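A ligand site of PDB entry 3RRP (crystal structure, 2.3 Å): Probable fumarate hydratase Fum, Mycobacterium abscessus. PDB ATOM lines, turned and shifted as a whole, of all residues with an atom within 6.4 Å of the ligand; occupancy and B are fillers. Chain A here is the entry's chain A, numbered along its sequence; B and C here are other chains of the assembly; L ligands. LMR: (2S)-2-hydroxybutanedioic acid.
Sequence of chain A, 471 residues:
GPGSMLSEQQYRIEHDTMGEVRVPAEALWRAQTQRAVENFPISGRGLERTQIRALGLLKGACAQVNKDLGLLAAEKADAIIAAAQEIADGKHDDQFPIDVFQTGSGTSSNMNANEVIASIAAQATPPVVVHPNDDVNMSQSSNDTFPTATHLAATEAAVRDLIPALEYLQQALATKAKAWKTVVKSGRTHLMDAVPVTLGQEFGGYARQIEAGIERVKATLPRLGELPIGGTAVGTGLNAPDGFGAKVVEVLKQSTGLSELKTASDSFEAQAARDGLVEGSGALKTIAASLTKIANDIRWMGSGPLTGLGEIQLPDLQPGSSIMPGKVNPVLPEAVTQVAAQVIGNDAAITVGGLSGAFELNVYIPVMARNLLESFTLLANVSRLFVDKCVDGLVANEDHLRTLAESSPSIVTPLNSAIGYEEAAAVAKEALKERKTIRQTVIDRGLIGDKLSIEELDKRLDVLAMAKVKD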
ATOM      1  N   THR A 103      13.625  25.794  -9.430  1.00  0.00           N
ATOM      2  CA  THR A 103      14.702  24.820  -9.628  1.00  0.00           C
ATOM      3  C   THR A 103      15.477  25.145 -10.899  1.00  0.00           C
ATOM      4  O   THR A 103      14.887  25.435 -11.951  1.00  0.00           O
ATOM      5  CB  THR A 103      14.170  23.352  -9.712  1.00  0.00           C
ATOM      6  OG1 THR A 103      15.284  22.462  -9.923  1.00  0.00           O
ATOM      7  CG2 THR A 103      13.121  23.173 -10.853  1.00  0.00           C
ATOM      8  N   SER A 105      17.094  23.806 -13.304  1.00  0.00           N
ATOM      9  CA  SER A 105      17.058  23.080 -14.580  1.00  0.00           C
ATOM     10  C   SER A 105      15.830  23.526 -15.386  1.00  0.00           C
ATOM     11  O   SER A 105      15.668  23.154 -16.568  1.00  0.00           O
ATOM     12  CB  SER A 105      16.938  21.592 -14.310  1.00  0.00           C
ATOM     13  OG  SER A 105      15.785  21.365 -13.489  1.00  0.00           O
ATOM     14  N   GLY A 106      14.978  24.316 -14.724  1.00  0.00           N
ATOM     15  CA  GLY A 106      13.633  24.558 -15.219  1.00  0.00           C
ATOM     16  C   GLY A 106      12.672  23.368 -15.213  1.00  0.00           C
ATOM     17  O   GLY A 106      11.740  23.319 -16.048  1.00  0.00           O
ATOM     18  N   THR A 107      12.854  22.405 -14.295  1.00  0.00           N
ATOM     19  CA  THR A 107      11.949  21.250 -14.232  1.00  0.00           C
ATOM     20  C   THR A 107      10.512  21.728 -14.137  1.00  0.00           C
ATOM     21  O   THR A 107       9.622  21.201 -14.799  1.00  0.00           O
ATOM     22  CB  THR A 107      12.229  20.314 -13.017  1.00  0.00           C
ATOM     23  OG1 THR A 107      13.584  19.840 -13.047  1.00  0.00           O
ATOM     24  CG2 THR A 107      11.231  19.131 -12.996  1.00  0.00           C
ATOM     25  N   SER A 108      10.296  22.754 -13.303  1.00  0.00           N
ATOM     26  CA  SER A 108       8.991  23.248 -12.999  1.00  0.00           C
ATOM     27  C   SER A 108       8.292  23.849 -14.218  1.00  0.00           C
ATOM     28  O   SER A 108       7.132  23.507 -14.470  1.00  0.00           O
ATOM     29  CB  SER A 108       9.073  24.252 -11.854  1.00  0.00           C
ATOM     30  OG  SER A 108       9.461  23.621 -10.634  1.00  0.00           O
ATOM     31  N   ASN A 110       9.130  23.261 -17.349  1.00  0.00           N
ATOM     32  CA  ASN A 110       8.940  22.166 -18.316  1.00  0.00           C
ATOM     33  C   ASN A 110       7.651  21.372 -18.007  1.00  0.00           C
ATOM     34  O   ASN A 110       6.862  21.077 -18.916  1.00  0.00           O
ATOM     35  CB  ASN A 110      10.166  21.249 -18.349  1.00  0.00           C
ATOM     36  CG  ASN A 110       9.987  20.077 -19.279  1.00  0.00           C
ATOM     37  OD1 ASN A 110       9.429  20.217 -20.363  1.00  0.00           O
ATOM     38  ND2 ASN A 110      10.483  18.901 -18.852  1.00  0.00           N
ATOM     39  N   MET A 111       7.436  21.081 -16.725  1.00  0.00           N
ATOM     40  CA  MET A 111       6.194  20.437 -16.240  1.00  0.00           C
ATOM     41  C   MET A 111       4.963  21.346 -16.406  1.00  0.00           C
ATOM     42  O   MET A 111       3.846  20.876 -16.675  1.00  0.00           O
ATOM     43  CB  MET A 111       6.358  20.017 -14.774  1.00  0.00           C
ATOM     44  CG  MET A 111       7.276  18.810 -14.550  1.00  0.00           C
ATOM     45  SD  MET A 111       7.092  17.471 -15.743  1.00  0.00           S
ATOM     46  CE  MET A 111       5.368  16.958 -15.548  1.00  0.00           C
ATOM     47  N   ASN A 137       5.930  14.832 -22.533  1.00  0.00           N
ATOM     48  CA  ASN A 137       7.387  14.808 -22.311  1.00  0.00           C
ATOM     49  C   ASN A 137       8.146  13.614 -22.964  1.00  0.00           C
ATOM     50  O   ASN A 137       9.341  13.388 -22.710  1.00  0.00           O
ATOM     51  CB  ASN A 137       7.698  14.887 -20.816  1.00  0.00           C
ATOM     52  CG  ASN A 137       9.015  15.497 -20.553  1.00  0.00           C
ATOM     53  OD1 ASN A 137       9.275  16.642 -20.939  1.00  0.00           O
ATOM     54  ND2 ASN A 137       9.889  14.751 -19.873  1.00  0.00           N
ATOM     55  N   GLN A 140      12.083  13.441 -23.840  1.00  0.00           N
ATOM     56  CA  GLN A 140      12.592  14.746 -23.409  1.00  0.00           C
ATOM     57  C   GLN A 140      13.007  14.680 -21.961  1.00  0.00           C
ATOM     58  O   GLN A 140      12.532  13.835 -21.209  1.00  0.00           O
ATOM     59  CB  GLN A 140      11.485  15.810 -23.550  1.00  0.00           C
ATOM     60  CG  GLN A 140      10.951  15.936 -24.966  1.00  0.00           C
ATOM     61  CD  GLN A 140       9.657  16.726 -25.034  1.00  0.00           C
ATOM     62  OE1 GLN A 140       9.622  17.898 -24.643  1.00  0.00           O
ATOM     63  NE2 GLN A 140       8.597  16.092 -25.518  1.00  0.00           N
ATOM     64  N   SER A 141      13.892  15.577 -21.581  1.00  0.00           N
ATOM     65  CA  SER A 141      14.123  15.864 -20.173  1.00  0.00           C
ATOM     66  C   SER A 141      13.934  17.359 -20.094  1.00  0.00           C
ATOM     67  O   SER A 141      13.803  18.000 -21.154  1.00  0.00           O
ATOM     68  CB  SER A 141      15.553  15.485 -19.804  1.00  0.00           C
ATOM     69  OG  SER A 141      15.908  16.013 -18.538  1.00  0.00           O
ATOM     70  N   SER A 142      13.894  17.907 -18.883  1.00  0.00           N
ATOM     71  CA  SER A 142      13.937  19.361 -18.715  1.00  0.00           C
ATOM     72  C   SER A 142      15.335  19.806 -19.056  1.00  0.00           C
ATOM     73  O   SER A 142      15.558  20.957 -19.426  1.00  0.00           O
ATOM     74  CB  SER A 142      13.671  19.786 -17.263  1.00  0.00           C
ATOM     75  OG  SER A 142      12.494  19.251 -16.712  1.00  0.00           O
ATOM     76  N   ASN A 143      16.282  18.888 -18.925  1.00  0.00           N
ATOM     77  CA  ASN A 143      17.692  19.234 -19.010  1.00  0.00           C
ATOM     78  C   ASN A 143      18.166  19.585 -20.382  1.00  0.00           C
ATOM     79  O   ASN A 143      19.187  20.260 -20.507  1.00  0.00           O
ATOM     80  CB  ASN A 143      18.552  18.141 -18.365  1.00  0.00           C
ATOM     81  CG  ASN A 143      18.271  18.029 -16.884  1.00  0.00           C
ATOM     82  OD1 ASN A 143      17.580  18.874 -16.331  1.00  0.00           O
ATOM     83  ND2 ASN A 143      18.792  16.993 -16.237  1.00  0.00           N
ATOM     84  N   ALA A 233      18.482  13.494 -20.196  1.00  0.00           N
ATOM     85  CA  ALA A 233      18.782  13.704 -18.777  1.00  0.00           C
ATOM     86  C   ALA A 233      20.202  14.152 -18.482  1.00  0.00           C
ATOM     87  O   ALA A 233      20.418  15.030 -17.631  1.00  0.00           O
ATOM     88  CB  ALA A 233      18.466  12.439 -17.975  1.00  0.00           C
ATOM     89  N   LEU A 361      25.027  18.911 -15.215  1.00  0.00           N
ATOM     90  CA  LEU A 361      24.005  19.938 -15.347  1.00  0.00           C
ATOM     91  C   LEU A 361      24.395  21.248 -14.696  1.00  0.00           C
ATOM     92  O   LEU A 361      24.726  21.286 -13.503  1.00  0.00           O
ATOM     93  CB  LEU A 361      22.682  19.449 -14.752  1.00  0.00           C
ATOM     94  CG  LEU A 361      21.437  20.307 -15.060  1.00  0.00           C
ATOM     95  CD1 LEU A 361      21.169  20.465 -16.608  1.00  0.00           C
ATOM     96  CD2 LEU A 361      20.205  19.717 -14.338  1.00  0.00           C
ATOM     97  N   VAL A 363      22.701  24.222 -13.189  1.00  0.00           N
ATOM     98  CA  VAL A 363      21.393  24.496 -12.644  1.00  0.00           C
ATOM     99  C   VAL A 363      21.199  25.995 -12.313  1.00  0.00           C
ATOM    100  O   VAL A 363      20.763  26.368 -11.220  1.00  0.00           O
ATOM    101  CB  VAL A 363      21.076  23.578 -11.450  1.00  0.00           C
ATOM    102  CG1 VAL A 363      20.868  22.157 -11.930  1.00  0.00           C
ATOM    103  CG2 VAL A 363      22.192  23.594 -10.438  1.00  0.00           C
ATOM    104  N   THR B 189      22.994  15.061 -11.671  1.00  0.00           N
ATOM    105  CA  THR B 189      22.381  16.348 -11.966  1.00  0.00           C
ATOM    106  C   THR B 189      21.789  16.918 -10.677  1.00  0.00           C
ATOM    107  O   THR B 189      21.081  16.193  -9.955  1.00  0.00           O
ATOM    108  CB  THR B 189      21.262  16.231 -13.029  1.00  0.00           C
ATOM    109  OG1 THR B 189      20.221  15.364 -12.556  1.00  0.00           O
ATOM    110  CG2 THR B 189      21.822  15.721 -14.329  1.00  0.00           C
ATOM    111  N   HIS B 190      22.064  18.196 -10.397  1.00  0.00           N
ATOM    112  CA  HIS B 190      21.631  18.855  -9.134  1.00  0.00           C
ATOM    113  C   HIS B 190      22.388  18.304  -7.948  1.00  0.00           C
ATOM    114  O   HIS B 190      21.999  18.540  -6.794  1.00  0.00           O
ATOM    115  CB  HIS B 190      20.120  18.673  -8.817  1.00  0.00           C
ATOM    116  CG  HIS B 190      19.194  19.138  -9.895  1.00  0.00           C
ATOM    117  ND1 HIS B 190      18.409  20.268  -9.764  1.00  0.00           N
ATOM    118  CD2 HIS B 190      18.867  18.593 -11.090  1.00  0.00           C
ATOM    119  CE1 HIS B 190      17.676  20.427 -10.849  1.00  0.00           C
ATOM    120  NE2 HIS B 190      17.919  19.411 -11.663  1.00  0.00           N
ATOM    121  N   MET B 192      22.502  15.203  -7.375  1.00  0.00           N
ATOM    122  CA  MET B 192      21.811  13.949  -7.058  1.00  0.00           C
ATOM    123  C   MET B 192      22.018  12.858  -8.115  1.00  0.00           C
ATOM    124  O   MET B 192      22.234  13.163  -9.295  1.00  0.00           O
ATOM    125  CB  MET B 192      20.307  14.201  -6.884  1.00  0.00           C
ATOM    126  CG  MET B 192      19.977  15.436  -6.034  1.00  0.00           C
ATOM    127  SD  MET B 192      20.759  15.280  -4.437  1.00  0.00           S
ATOM    128  CE  MET B 192      19.584  14.292  -3.535  1.00  0.00           C
ATOM    129  N   ALA B 194      21.912  10.587 -10.949  1.00  0.00           N
ATOM    130  CA  ALA B 194      21.183  10.593 -12.216  1.00  0.00           C
ATOM    131  C   ALA B 194      21.353   9.243 -12.895  1.00  0.00           C
ATOM    132  O   ALA B 194      21.371   8.212 -12.234  1.00  0.00           O
ATOM    133  CB  ALA B 194      21.658  11.740 -13.100  1.00  0.00           C
ATOM    134  N   GLY C 320      11.585  15.836  -8.539  1.00  0.00           N
ATOM    135  CA  GLY C 320      12.803  16.395  -9.125  1.00  0.00           C
ATOM    136  C   GLY C 320      12.825  16.347 -10.652  1.00  0.00           C
ATOM    137  O   GLY C 320      13.265  17.287 -11.291  1.00  0.00           O
ATOM    138  N   SER C 321      12.330  15.270 -11.263  1.00  0.00           N
ATOM    139  CA  SER C 321      12.655  15.054 -12.683  1.00  0.00           C
ATOM    140  C   SER C 321      11.486  14.663 -13.554  1.00  0.00           C
ATOM    141  O   SER C 321      10.704  13.782 -13.211  1.00  0.00           O
ATOM    142  CB  SER C 321      13.792  14.048 -12.823  1.00  0.00           C
ATOM    143  OG  SER C 321      14.061  13.762 -14.183  1.00  0.00           O
ATOM    144  N   SER C 322      11.347  15.331 -14.688  1.00  0.00           N
ATOM    145  CA  SER C 322      10.304  14.978 -15.634  1.00  0.00           C
ATOM    146  C   SER C 322      10.563  13.595 -16.272  1.00  0.00           C
ATOM    147  O   SER C 322       9.638  12.990 -16.838  1.00  0.00           O
ATOM    148  CB  SER C 322      10.194  16.065 -16.703  1.00  0.00           C
ATOM    149  OG  SER C 322      11.321  16.059 -17.555  1.00  0.00           O
ATOM    150  N   ILE C 323      11.813  13.115 -16.184  1.00  0.00           N
ATOM    151  CA  ILE C 323      12.270  11.893 -16.856  1.00  0.00           C
ATOM    152  C   ILE C 323      12.842  10.825 -15.929  1.00  0.00           C
ATOM    153  O   ILE C 323      12.681   9.633 -16.184  1.00  0.00           O
ATOM    154  CB  ILE C 323      13.308  12.199 -18.011  1.00  0.00           C
ATOM    155  CG1 ILE C 323      13.585  10.932 -18.845  1.00  0.00           C
ATOM    156  CG2 ILE C 323      14.616  12.836 -17.472  1.00  0.00           C
ATOM    157  CD1 ILE C 323      14.450  11.191 -20.106  1.00  0.00           C
ATOM    158  N   MET C 324      13.532  11.244 -14.880  1.00  0.00           N
ATOM    159  CA  MET C 324      14.127  10.301 -13.950  1.00  0.00           C
ATOM    160  C   MET C 324      13.163  10.098 -12.770  1.00  0.00           C
ATOM    161  O   MET C 324      13.039  10.954 -11.923  1.00  0.00           O
ATOM    162  CB  MET C 324      15.508  10.812 -13.479  1.00  0.00           C
ATOM    163  CG  MET C 324      16.608  10.671 -14.533  1.00  0.00           C
ATOM    164  SD  MET C 324      18.237  11.348 -14.124  1.00  0.00           S
ATOM    165  CE  MET C 324      17.924  13.125 -14.225  1.00  0.00           C
ATOM    166  N   LYS C 327      13.418  10.585  -8.453  1.00  0.00           N
ATOM    167  CA  LYS C 327      14.506  11.474  -8.093  1.00  0.00           C
ATOM    168  C   LYS C 327      13.955  12.759  -7.461  1.00  0.00           C
ATOM    169  O   LYS C 327      12.918  13.294  -7.897  1.00  0.00           O
ATOM    170  CB  LYS C 327      15.350  11.767  -9.336  1.00  0.00           C
ATOM    171  CG  LYS C 327      16.515  12.701  -9.121  1.00  0.00           C
ATOM    172  CD  LYS C 327      17.494  12.586 -10.290  1.00  0.00           C
ATOM    173  CE  LYS C 327      18.776  13.359 -10.000  1.00  0.00           C
ATOM    174  NZ  LYS C 327      18.717  14.796 -10.407  1.00  0.00           N
ATOM    175  N   VAL C 328      14.616  13.228  -6.410  1.00  0.00           N
ATOM    176  CA  VAL C 328      14.287  14.523  -5.824  1.00  0.00           C
ATOM    177  C   VAL C 328      15.542  15.399  -5.814  1.00  0.00           C
ATOM    178  O   VAL C 328      16.645  14.912  -5.599  1.00  0.00           O
ATOM    179  CB  VAL C 328      13.671  14.370  -4.404  1.00  0.00           C
ATOM    180  CG1 VAL C 328      13.162  15.727  -3.866  1.00  0.00           C
ATOM    181  CG2 VAL C 328      12.491  13.391  -4.437  1.00  0.00           C
ATOM    182  N   ASN C 329      15.353  16.712  -6.044  1.00  0.00           N
ATOM    183  CA  ASN C 329      16.464  17.661  -6.135  1.00  0.00           C
ATOM    184  C   ASN C 329      16.396  18.787  -5.119  1.00  0.00           C
ATOM    185  O   ASN C 329      15.302  19.200  -4.747  1.00  0.00           O
ATOM    186  CB  ASN C 329      16.551  18.240  -7.535  1.00  0.00           C
ATOM    187  CG  ASN C 329      16.741  17.167  -8.579  1.00  0.00           C
ATOM    188  OD1 ASN C 329      17.549  16.253  -8.400  1.00  0.00           O
ATOM    189  ND2 ASN C 329      16.020  17.260  -9.684  1.00  0.00           N
HETATM  190  C1  LMR L   1      16.997  16.394 -13.027  1.00  0.00           C
HETATM  191  O1A LMR L   1      16.806  15.790 -11.936  1.00  0.00           O
HETATM  192  O1B LMR L   1      18.142  16.450 -13.528  1.00  0.00           O
HETATM  193  C2  LMR L   1      15.852  17.089 -13.716  1.00  0.00           C
HETATM  194  O2  LMR L   1      16.237  18.440 -13.926  1.00  0.00           O
HETATM  195  C3  LMR L   1      15.566  16.421 -15.067  1.00  0.00           C
HETATM  196  C4  LMR L   1      14.182  16.778 -15.583  1.00  0.00           C
HETATM  197  O4A LMR L   1      13.861  16.352 -16.700  1.00  0.00           O
HETATM  198  O4B LMR L   1      13.352  17.481 -14.943  1.00  0.00           O
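The side-chain hydroxyl of Ser 142 is in hydrogen-bond range of an oxygen (O4B) of the ligand (2.6 Å).
O1A of the ligand is in hydrogen-bond range of ND2 of Asn 329 of chain C (2.8 Å).
OD1 of Asn 143 lies within hydrogen-bond range of O2 of the ligand, at 2.8 Å.
An oxygen (O4A) of the ligand is in hydrogen-bond range of the backbone NH of Ser 142 (2.7 Å).
O4A of the ligand is in hydrogen-bond range of OG of Ser 141.
The side-chain hydroxyl of Ser 322 of chain C lies within hydrogen-bond range of an oxygen (O4A) of the ligand, 2.7 Å away.
O1B of the ligand is in hydrogen-bond range of OG1 of Thr 189 of chain B, at 2.5 Å.
A ring nitrogen (NE2) of His 190 of chain B lies within hydrogen-bond range of an oxygen (O2) of the ligand, 3.0 Å away.
An oxygen (O2) of the ligand is in hydrogen-bond range of the side-chain hydroxyl of Ser 105, at 3.0 Å.
The side-chain hydroxyl of Thr 107 is in hydrogen-bond range of an oxygen (O4B) of the ligand (3.0 Å).
O4B of the ligand is in hydrogen-bond range of N of Ser 322 of chain C.
O1A of the ligand lies within salt-bridge range of NZ of Lys 327 of chain C, at 2.6 Å.
The backbone carbonyl oxygen (O) of Ala 233 is in hydrogen-bond range of the side-chain amide nitrogen (ND2) of Asn 143 (2.9 Å).
The side-chain hydroxyl (OG) of Ser 105 is in hydrogen-bond range of the side-chain hydroxyl (OG1) of Thr 107 (2.7 Å).
OD1 of Asn 329 of chain C lies within hydrogen-bond range of NZ of Lys 327 of chain C, at 2.7 Å.
The side-chain hydroxyl (OG) of Ser 142 is in hydrogen-bond range of the side-chain amide nitrogen (ND2) of Asn 110 (3.0 Å).
The side-chain amide nitrogen (ND2) of Asn 110 lies within hydrogen-bond range of the side-chain hydroxyl (OG) of Ser 322 of chain C, at 3.2 Å.
N of Met 324 of chain C sits at hydrogen-bond distance from OG of Ser 321 of chain C (2.7 Å).
O of Lys 327 of chain C lies within hydrogen-bond range of N of Gly 320 of chain C (2.9 Å).
The side-chain amide nitrogen (ND2) of Asn 137 is in hydrogen-bond range of the side-chain hydroxyl (OG) of Ser 322 of chain C, 3.0 Å away.
Merely in contact with the ligand: Ser 321 of chain C, Met 324 of chain C, Gly 320 of chain C, Ile 323 of chain C and Leu 361.
15 residues have an atom within 4 Å of the ligand: Ser 105, Thr 107, Ser 141, Ser 142, Asn 143, Leu 361, Thr 189 of chain B, His 190 of chain B, Gly 320 of chain C, Ser 321 of chain C, Ser 322 of chain C, Ile 323 of chain C, Met 324 of chain C, Lys 327 of chain C and Asn 329 of chain C.
Along chain A the residues within 4 Å of the ligand span positions 105 to 361.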
